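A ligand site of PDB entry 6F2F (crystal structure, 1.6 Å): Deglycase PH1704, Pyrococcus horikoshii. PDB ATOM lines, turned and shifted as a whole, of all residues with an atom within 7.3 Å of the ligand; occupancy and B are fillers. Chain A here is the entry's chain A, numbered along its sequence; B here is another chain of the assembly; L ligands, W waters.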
ATOM      1  N   THR A   7     -19.805 -21.957  19.304  1.00  0.00           N
ATOM      2  CA  THR A   7     -18.545 -22.025  18.541  1.00  0.00           C
ATOM      3  C   THR A   7     -17.532 -21.037  19.127  1.00  0.00           C
ATOM      4  O   THR A   7     -17.753 -20.463  20.205  1.00  0.00           O
ATOM      5  CB  THR A   7     -18.874 -21.772  17.080  1.00  0.00           C
ATOM      6  OG1 THR A   7     -17.725 -22.013  16.270  1.00  0.00           O
ATOM      7  CG2 THR A   7     -19.360 -20.375  16.835  1.00  0.00           C
ATOM      8  N   ALA A   8     -16.406 -20.910  18.475  1.00  0.00           N
ATOM      9  CA  ALA A   8     -15.277 -20.109  18.973  1.00  0.00           C
ATOM     10  C   ALA A   8     -14.284 -19.922  17.832  1.00  0.00           C
ATOM     11  O   ALA A   8     -14.508 -20.368  16.687  1.00  0.00           O
ATOM     12  CB  ALA A   8     -14.622 -20.866  20.147  1.00  0.00           C
ATOM     13  N   ASN A   9     -13.211 -19.193  18.090  1.00  0.00           N
ATOM     14  CA  ASN A   9     -12.154 -19.085  17.107  1.00  0.00           C
ATOM     15  C   ASN A   9     -11.663 -20.464  16.661  1.00  0.00           C
ATOM     16  O   ASN A   9     -11.691 -21.443  17.398  1.00  0.00           O
ATOM     17  CB  ASN A   9     -10.969 -18.286  17.666  1.00  0.00           C
ATOM     18  CG  ASN A   9     -11.238 -16.807  17.725  1.00  0.00           C
ATOM     19  OD1 ASN A   9     -11.818 -16.206  16.804  1.00  0.00           O
ATOM     20  ND2 ASN A   9     -10.797 -16.148  18.782  1.00  0.00           N
ATOM     21  N   GLU A  10     -11.218 -20.522  15.385  1.00  0.00           N
ATOM     22  CA  GLU A  10     -10.711 -21.750  14.756  1.00  0.00           C
ATOM     23  C   GLU A  10     -11.808 -22.744  14.474  1.00  0.00           C
ATOM     24  O   GLU A  10     -11.573 -23.925  14.293  1.00  0.00           O
ATOM     25  CB  GLU A  10      -9.524 -22.370  15.502  1.00  0.00           C
ATOM     26  CG  GLU A  10      -8.399 -21.363  15.746  1.00  0.00           C
ATOM     27  CD  GLU A  10      -7.789 -20.751  14.508  1.00  0.00           C
ATOM     28  OE1 GLU A  10      -7.548 -19.527  14.486  1.00  0.00           O
ATOM     29  OE2 GLU A  10      -7.598 -21.496  13.518  1.00  0.00           O
ATOM     30  N   SER A  34     -20.501 -17.305  21.568  1.00  0.00           N
ATOM     31  CA  SER A  34     -19.108 -17.631  21.824  1.00  0.00           C
ATOM     32  C   SER A  34     -18.649 -17.018  23.158  1.00  0.00           C
ATOM     33  O   SER A  34     -19.456 -16.558  23.964  1.00  0.00           O
ATOM     34  CB  SER A  34     -18.226 -17.222  20.647  1.00  0.00           C
ATOM     35  OG  SER A  34     -16.948 -17.838  20.781  1.00  0.00           O
ATOM     36  N   PHE A  35     -17.343 -17.017  23.389  1.00  0.00           N
ATOM     37  CA  PHE A  35     -16.814 -16.545  24.684  1.00  0.00           C
ATOM     38  C   PHE A  35     -17.075 -15.074  24.935  1.00  0.00           C
ATOM     39  O   PHE A  35     -17.338 -14.685  26.087  1.00  0.00           O
ATOM     40  CB  PHE A  35     -15.298 -16.794  24.753  1.00  0.00           C
ATOM     41  CG  PHE A  35     -14.951 -18.253  24.811  1.00  0.00           C
ATOM     42  CD1 PHE A  35     -14.925 -18.922  26.020  1.00  0.00           C
ATOM     43  CD2 PHE A  35     -14.624 -18.961  23.665  1.00  0.00           C
ATOM     44  CE1 PHE A  35     -14.591 -20.271  26.070  1.00  0.00           C
ATOM     45  CE2 PHE A  35     -14.318 -20.315  23.714  1.00  0.00           C
ATOM     46  CZ  PHE A  35     -14.302 -20.964  24.918  1.00  0.00           C
ATOM     47  N   GLU A  36     -16.947 -14.265  23.898  1.00  0.00           N
ATOM     48  CA  GLU A  36     -17.083 -12.808  23.974  1.00  0.00           C
ATOM     49  C   GLU A  36     -17.777 -12.269  22.785  1.00  0.00           C
ATOM     50  O   GLU A  36     -17.661 -12.813  21.683  1.00  0.00           O
ATOM     51  CB  GLU A  36     -15.697 -12.163  24.002  1.00  0.00           C
ATOM     52  CG  GLU A  36     -14.821 -12.556  25.181  1.00  0.00           C
ATOM     53  CD  GLU A  36     -13.487 -11.823  25.196  1.00  0.00           C
ATOM     54  OE1 GLU A  36     -13.171 -11.108  24.222  1.00  0.00           O
ATOM     55  OE2 GLU A  36     -12.731 -12.013  26.172  1.00  0.00           O
ATOM     56  N   ARG A  37     -18.347 -11.060  22.950  1.00  0.00           N
ATOM     57  CA  ARG A  37     -18.925 -10.377  21.812  1.00  0.00           C
ATOM     58  C   ARG A  37     -17.775  -9.815  20.953  1.00  0.00           C
ATOM     59  O   ARG A  37     -16.619  -9.785  21.374  1.00  0.00           O
ATOM     60  CB  ARG A  37     -19.922  -9.298  22.254  1.00  0.00           C
ATOM     61  CG  ARG A  37     -21.228  -9.915  22.774  1.00  0.00           C
ATOM     62  CD  ARG A  37     -22.497  -9.170  22.410  1.00  0.00           C
ATOM     63  NE  ARG A  37     -22.658  -7.947  23.204  1.00  0.00           N
ATOM     64  CZ  ARG A  37     -23.793  -7.256  23.300  1.00  0.00           C
ATOM     65  NH1 ARG A  37     -24.896  -7.648  22.662  1.00  0.00           N
ATOM     66  NH2 ARG A  37     -23.844  -6.147  24.039  1.00  0.00           N
ATOM     67  N   GLY A  38     -18.111  -9.424  19.746  1.00  0.00           N
ATOM     68  CA  GLY A  38     -17.154  -8.994  18.747  1.00  0.00           C
ATOM     69  C   GLY A  38     -17.192  -9.992  17.601  1.00  0.00           C
ATOM     70  O   GLY A  38     -18.273 -10.355  17.163  1.00  0.00           O
ATOM     71  N   THR A  39     -16.033 -10.450  17.145  1.00  0.00           N
ATOM     72  CA  THR A  39     -15.948 -11.380  16.034  1.00  0.00           C
ATOM     73  C   THR A  39     -15.115 -12.585  16.443  1.00  0.00           C
ATOM     74  O   THR A  39     -14.354 -12.531  17.418  1.00  0.00           O
ATOM     75  CB  THR A  39     -15.359 -10.724  14.774  1.00  0.00           C
ATOM     76  OG1 THR A  39     -14.006 -10.425  15.026  1.00  0.00           O
ATOM     77  CG2 THR A  39     -16.107  -9.465  14.356  1.00  0.00           C
ATOM     78  N   ILE A  40     -15.328 -13.672  15.717  1.00  0.00           N
ATOM     79  CA  ILE A  40     -14.536 -14.886  15.777  1.00  0.00           C
ATOM     80  C   ILE A  40     -14.069 -15.152  14.356  1.00  0.00           C
ATOM     81  O   ILE A  40     -14.721 -14.740  13.396  1.00  0.00           O
ATOM     82  CB  ILE A  40     -15.247 -16.087  16.434  1.00  0.00           C
ATOM     83  CG1 ILE A  40     -16.630 -16.291  15.833  1.00  0.00           C
ATOM     84  CG2 ILE A  40     -15.313 -15.873  17.938  1.00  0.00           C
ATOM     85  CD1 ILE A  40     -17.278 -17.610  16.191  1.00  0.00           C
ATOM     86  N   THR A  41     -12.937 -15.856  14.216  1.00  0.00           N
ATOM     87  CA  THR A  41     -12.297 -16.110  12.931  1.00  0.00           C
ATOM     88  C   THR A  41     -12.087 -17.598  12.758  1.00  0.00           C
ATOM     89  O   THR A  41     -11.569 -18.253  13.667  1.00  0.00           O
ATOM     90  CB  THR A  41     -10.979 -15.337  12.812  1.00  0.00           C
ATOM     91  OG1 THR A  41     -11.244 -13.956  13.024  1.00  0.00           O
ATOM     92  CG2 THR A  41     -10.316 -15.506  11.453  1.00  0.00           C
ATOM     93  N   VAL A  50     -20.208 -12.375  16.604  1.00  0.00           N
ATOM     94  CA  VAL A  50     -20.776 -13.081  17.731  1.00  0.00           C
ATOM     95  C   VAL A  50     -22.035 -12.301  18.172  1.00  0.00           C
ATOM     96  O   VAL A  50     -21.945 -11.106  18.440  1.00  0.00           O
ATOM     97  CB  VAL A  50     -19.781 -13.206  18.895  1.00  0.00           C
ATOM     98  CG1 VAL A  50     -20.442 -13.820  20.133  1.00  0.00           C
ATOM     99  CG2 VAL A  50     -18.553 -14.017  18.468  1.00  0.00           C
ATOM    100  N   PHE A  54     -21.702 -16.986  25.845  1.00  0.00           N
ATOM    101  CA  PHE A  54     -22.254 -18.186  26.493  1.00  0.00           C
ATOM    102  C   PHE A  54     -22.989 -17.806  27.793  1.00  0.00           C
ATOM    103  O   PHE A  54     -24.068 -18.346  28.074  1.00  0.00           O
ATOM    104  CB  PHE A  54     -21.138 -19.190  26.832  1.00  0.00           C
ATOM    105  CG  PHE A  54     -20.353 -19.678  25.643  1.00  0.00           C
ATOM    106  CD1 PHE A  54     -20.999 -20.138  24.503  1.00  0.00           C
ATOM    107  CD2 PHE A  54     -18.968 -19.797  25.707  1.00  0.00           C
ATOM    108  CE1 PHE A  54     -20.264 -20.655  23.440  1.00  0.00           C
ATOM    109  CE2 PHE A  54     -18.250 -20.340  24.649  1.00  0.00           C
ATOM    110  CZ  PHE A  54     -18.896 -20.769  23.536  1.00  0.00           C
ATOM    111  N   ALA A  72     -12.390 -25.294  17.345  1.00  0.00           N
ATOM    112  CA  ALA A  72     -13.230 -24.569  18.297  1.00  0.00           C
ATOM    113  C   ALA A  72     -13.881 -25.470  19.333  1.00  0.00           C
ATOM    114  O   ALA A  72     -13.924 -25.104  20.511  1.00  0.00           O
ATOM    115  CB  ALA A  72     -14.306 -23.771  17.568  1.00  0.00           C
ATOM    116  N   GLU A  74     -12.844 -28.026  21.006  1.00  0.00           N
ATOM    117  CA  GLU A  74     -11.968 -28.322  22.144  1.00  0.00           C
ATOM    118  C   GLU A  74     -11.830 -27.117  23.088  1.00  0.00           C
ATOM    119  O   GLU A  74     -11.535 -27.311  24.264  1.00  0.00           O
ATOM    120  CB  GLU A  74     -10.592 -28.878  21.720  1.00  0.00           C
ATOM    121  CG  GLU A  74     -10.728 -30.369  21.421  1.00  0.00           C
ATOM    122  CD  GLU A  74      -9.497 -31.034  20.820  1.00  0.00           C
ATOM    123  OE1 GLU A  74      -8.416 -30.528  21.175  1.00  0.00           O
ATOM    124  OE2 GLU A  74      -9.587 -31.975  19.993  1.00  0.00           O
ATOM    125  N   ARG A  75     -12.099 -25.912  22.621  1.00  0.00           N
ATOM    126  CA  ARG A  75     -12.141 -24.721  23.469  1.00  0.00           C
ATOM    127  C   ARG A  75     -13.536 -24.641  24.152  1.00  0.00           C
ATOM    128  O   ARG A  75     -13.655 -24.466  25.372  1.00  0.00           O
ATOM    129  CB  ARG A  75     -11.922 -23.428  22.665  1.00  0.00           C
ATOM    130  CG  ARG A  75     -10.664 -23.419  21.774  1.00  0.00           C
ATOM    131  CD  ARG A  75     -10.489 -22.044  21.140  1.00  0.00           C
ATOM    132  NE  ARG A  75      -9.297 -21.998  20.298  1.00  0.00           N
ATOM    133  CZ  ARG A  75      -8.595 -20.915  19.994  1.00  0.00           C
ATOM    134  NH1 ARG A  75      -8.980 -19.720  20.433  1.00  0.00           N
ATOM    135  NH2 ARG A  75      -7.538 -21.013  19.224  1.00  0.00           N
ATOM    136  N   VAL A  76     -14.593 -24.770  23.344  1.00  0.00           N
ATOM    137  CA  VAL A  76     -15.968 -24.673  23.827  1.00  0.00           C
ATOM    138  C   VAL A  76     -16.227 -25.693  24.943  1.00  0.00           C
ATOM    139  O   VAL A  76     -16.899 -25.391  25.931  1.00  0.00           O
ATOM    140  CB  VAL A  76     -16.981 -24.814  22.690  1.00  0.00           C
ATOM    141  CG1 VAL A  76     -18.412 -24.769  23.192  1.00  0.00           C
ATOM    142  CG2 VAL A  76     -16.749 -23.739  21.637  1.00  0.00           C
ATOM    143  N   LEU A  78     -14.457 -26.836  27.237  1.00  0.00           N
ATOM    144  CA  LEU A  78     -13.900 -26.522  28.541  1.00  0.00           C
ATOM    145  C   LEU A  78     -14.652 -25.380  29.222  1.00  0.00           C
ATOM    146  O   LEU A  78     -14.350 -25.053  30.374  1.00  0.00           O
ATOM    147  CB  LEU A  78     -12.435 -26.124  28.416  1.00  0.00           C
ATOM    148  CG  LEU A  78     -11.481 -27.262  28.043  1.00  0.00           C
ATOM    149  CD1 LEU A  78     -10.107 -26.732  27.832  1.00  0.00           C
ATOM    150  CD2 LEU A  78     -11.474 -28.306  29.093  1.00  0.00           C
ATOM    151  N   ASN A  79     -15.657 -24.793  28.552  1.00  0.00           N
ATOM    152  CA  ASN A  79     -16.483 -23.741  29.143  1.00  0.00           C
ATOM    153  C   ASN A  79     -17.695 -24.412  29.723  1.00  0.00           C
ATOM    154  O   ASN A  79     -18.540 -24.946  29.006  1.00  0.00           O
ATOM    155  CB  ASN A  79     -16.862 -22.743  28.081  1.00  0.00           C
ATOM    156  CG  ASN A  79     -17.622 -21.571  28.646  1.00  0.00           C
ATOM    157  OD1 ASN A  79     -18.836 -21.649  28.766  1.00  0.00           O
ATOM    158  ND2 ASN A  79     -16.952 -20.515  29.051  1.00  0.00           N
ATOM    159  N   TYR B 120      -3.473 -32.502  26.960  1.00  0.00           N
ATOM    160  CA  TYR B 120      -4.049 -31.196  26.686  1.00  0.00           C
ATOM    161  C   TYR B 120      -5.401 -31.205  27.412  1.00  0.00           C
ATOM    162  O   TYR B 120      -6.178 -32.168  27.281  1.00  0.00           O
ATOM    163  CB  TYR B 120      -4.291 -31.058  25.181  1.00  0.00           C
ATOM    164  CG  TYR B 120      -4.897 -29.727  24.830  1.00  0.00           C
ATOM    165  CD1 TYR B 120      -4.208 -28.542  25.089  1.00  0.00           C
ATOM    166  CD2 TYR B 120      -6.090 -29.648  24.136  1.00  0.00           C
ATOM    167  CE1 TYR B 120      -4.762 -27.303  24.770  1.00  0.00           C
ATOM    168  CE2 TYR B 120      -6.661 -28.401  23.829  1.00  0.00           C
ATOM    169  CZ  TYR B 120      -5.975 -27.243  24.112  1.00  0.00           C
ATOM    170  OH  TYR B 120      -6.508 -26.012  23.813  1.00  0.00           O
HETATM  171  C1  LIG L   1     -13.343 -16.145  21.323  1.00  0.00           C
HETATM  172  C2  LIG L   1     -10.318 -19.977  25.131  1.00  0.00           C
HETATM  173  C3  LIG L   1     -11.663 -14.611  22.863  1.00  0.00           C
HETATM  174  C4  LIG L   1     -11.617 -16.512  25.799  1.00  0.00           C
HETATM  175  C5  LIG L   1     -11.068 -15.058  25.837  1.00  0.00           C
HETATM  176  C6  LIG L   1      -9.714 -17.600  26.912  1.00  0.00           C
HETATM  177  C7  LIG L   1      -8.211 -17.478  26.556  1.00  0.00           C
HETATM  178  C8  LIG L   1      -7.971 -15.107  26.098  1.00  0.00           C
HETATM  179  C9  LIG L   1      -8.853 -14.105  25.340  1.00  0.00           C
HETATM  180  C10 LIG L   1     -10.342 -21.341  25.391  1.00  0.00           C
HETATM  181  C11 LIG L   1      -9.355 -22.155  24.901  1.00  0.00           C
HETATM  182  C12 LIG L   1      -8.328 -21.618  24.159  1.00  0.00           C
HETATM  183  C13 LIG L   1      -8.337 -20.241  23.953  1.00  0.00           C
HETATM  184  C14 LIG L   1      -7.387 -19.381  23.176  1.00  0.00           C
HETATM  185  C15 LIG L   1     -12.833 -14.065  22.347  1.00  0.00           C
HETATM  186  C16 LIG L   1     -13.667 -14.843  21.580  1.00  0.00           C
HETATM  187  C17 LIG L   1     -12.167 -16.652  21.867  1.00  0.00           C
HETATM  188  C18 LIG L   1     -11.742 -18.079  21.626  1.00  0.00           C
HETATM  189  C19 LIG L   1     -10.646 -13.832  23.723  1.00  0.00           C
HETATM  190  C20 LIG L   1     -11.323 -18.896  25.595  1.00  0.00           C
HETATM  191  N1  LIG L   1     -10.585 -17.592  25.714  1.00  0.00           N
HETATM  192  N2  LIG L   1      -7.955 -16.463  25.532  1.00  0.00           N
HETATM  193  N3  LIG L   1     -10.068 -14.730  24.766  1.00  0.00           N
HETATM  194  N4  LIG L   1      -9.327 -19.480  24.412  1.00  0.00           N
HETATM  195  N5  LIG L   1     -11.350 -15.896  22.620  1.00  0.00           N
HETATM  196  O1  LIG L   1     -12.386 -18.747  20.821  1.00  0.00           O
HETATM  197  O2  LIG L   1     -10.771 -18.545  22.249  1.00  0.00           O
HETATM  198  O3  LIG L   1      -6.371 -19.909  22.643  1.00  0.00           O
HETATM  199  O4  LIG L   1      -7.813 -18.163  23.109  1.00  0.00           O
HETATM  200 TB1  LIG L   1      -9.333 -17.069  23.460  1.00  0.00          TB
HETATM  201  O   HOH W   1     -12.590 -22.811  27.333  1.00  0.00           O
HETATM  202  O   HOH W   2     -15.151 -12.445  20.086  1.00  0.00           O
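Merely in contact with the ligand: Ala 8, Glu 36, Phe 35 and Ile 40. Hydrophobic or aromatic side chains within 4 Å of the ligand: Ala 8, Phe 35 and Ile 40. Within 4 Å of the ligand: Ala 8, Asn 9, Phe 35, Glu 36, Ile 40 and Arg 75.
O3 of the ligand lies within salt-bridge range of NH1 of Arg 75, 3.4 Å away. The backbone NH (N) of Asn 9 lies within hydrogen-bond range of an oxygen (O1) of the ligand, 2.9 Å away.
OD1 of Asn 9 is in hydrogen-bond range of N of Thr 41 (2.8 Å).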
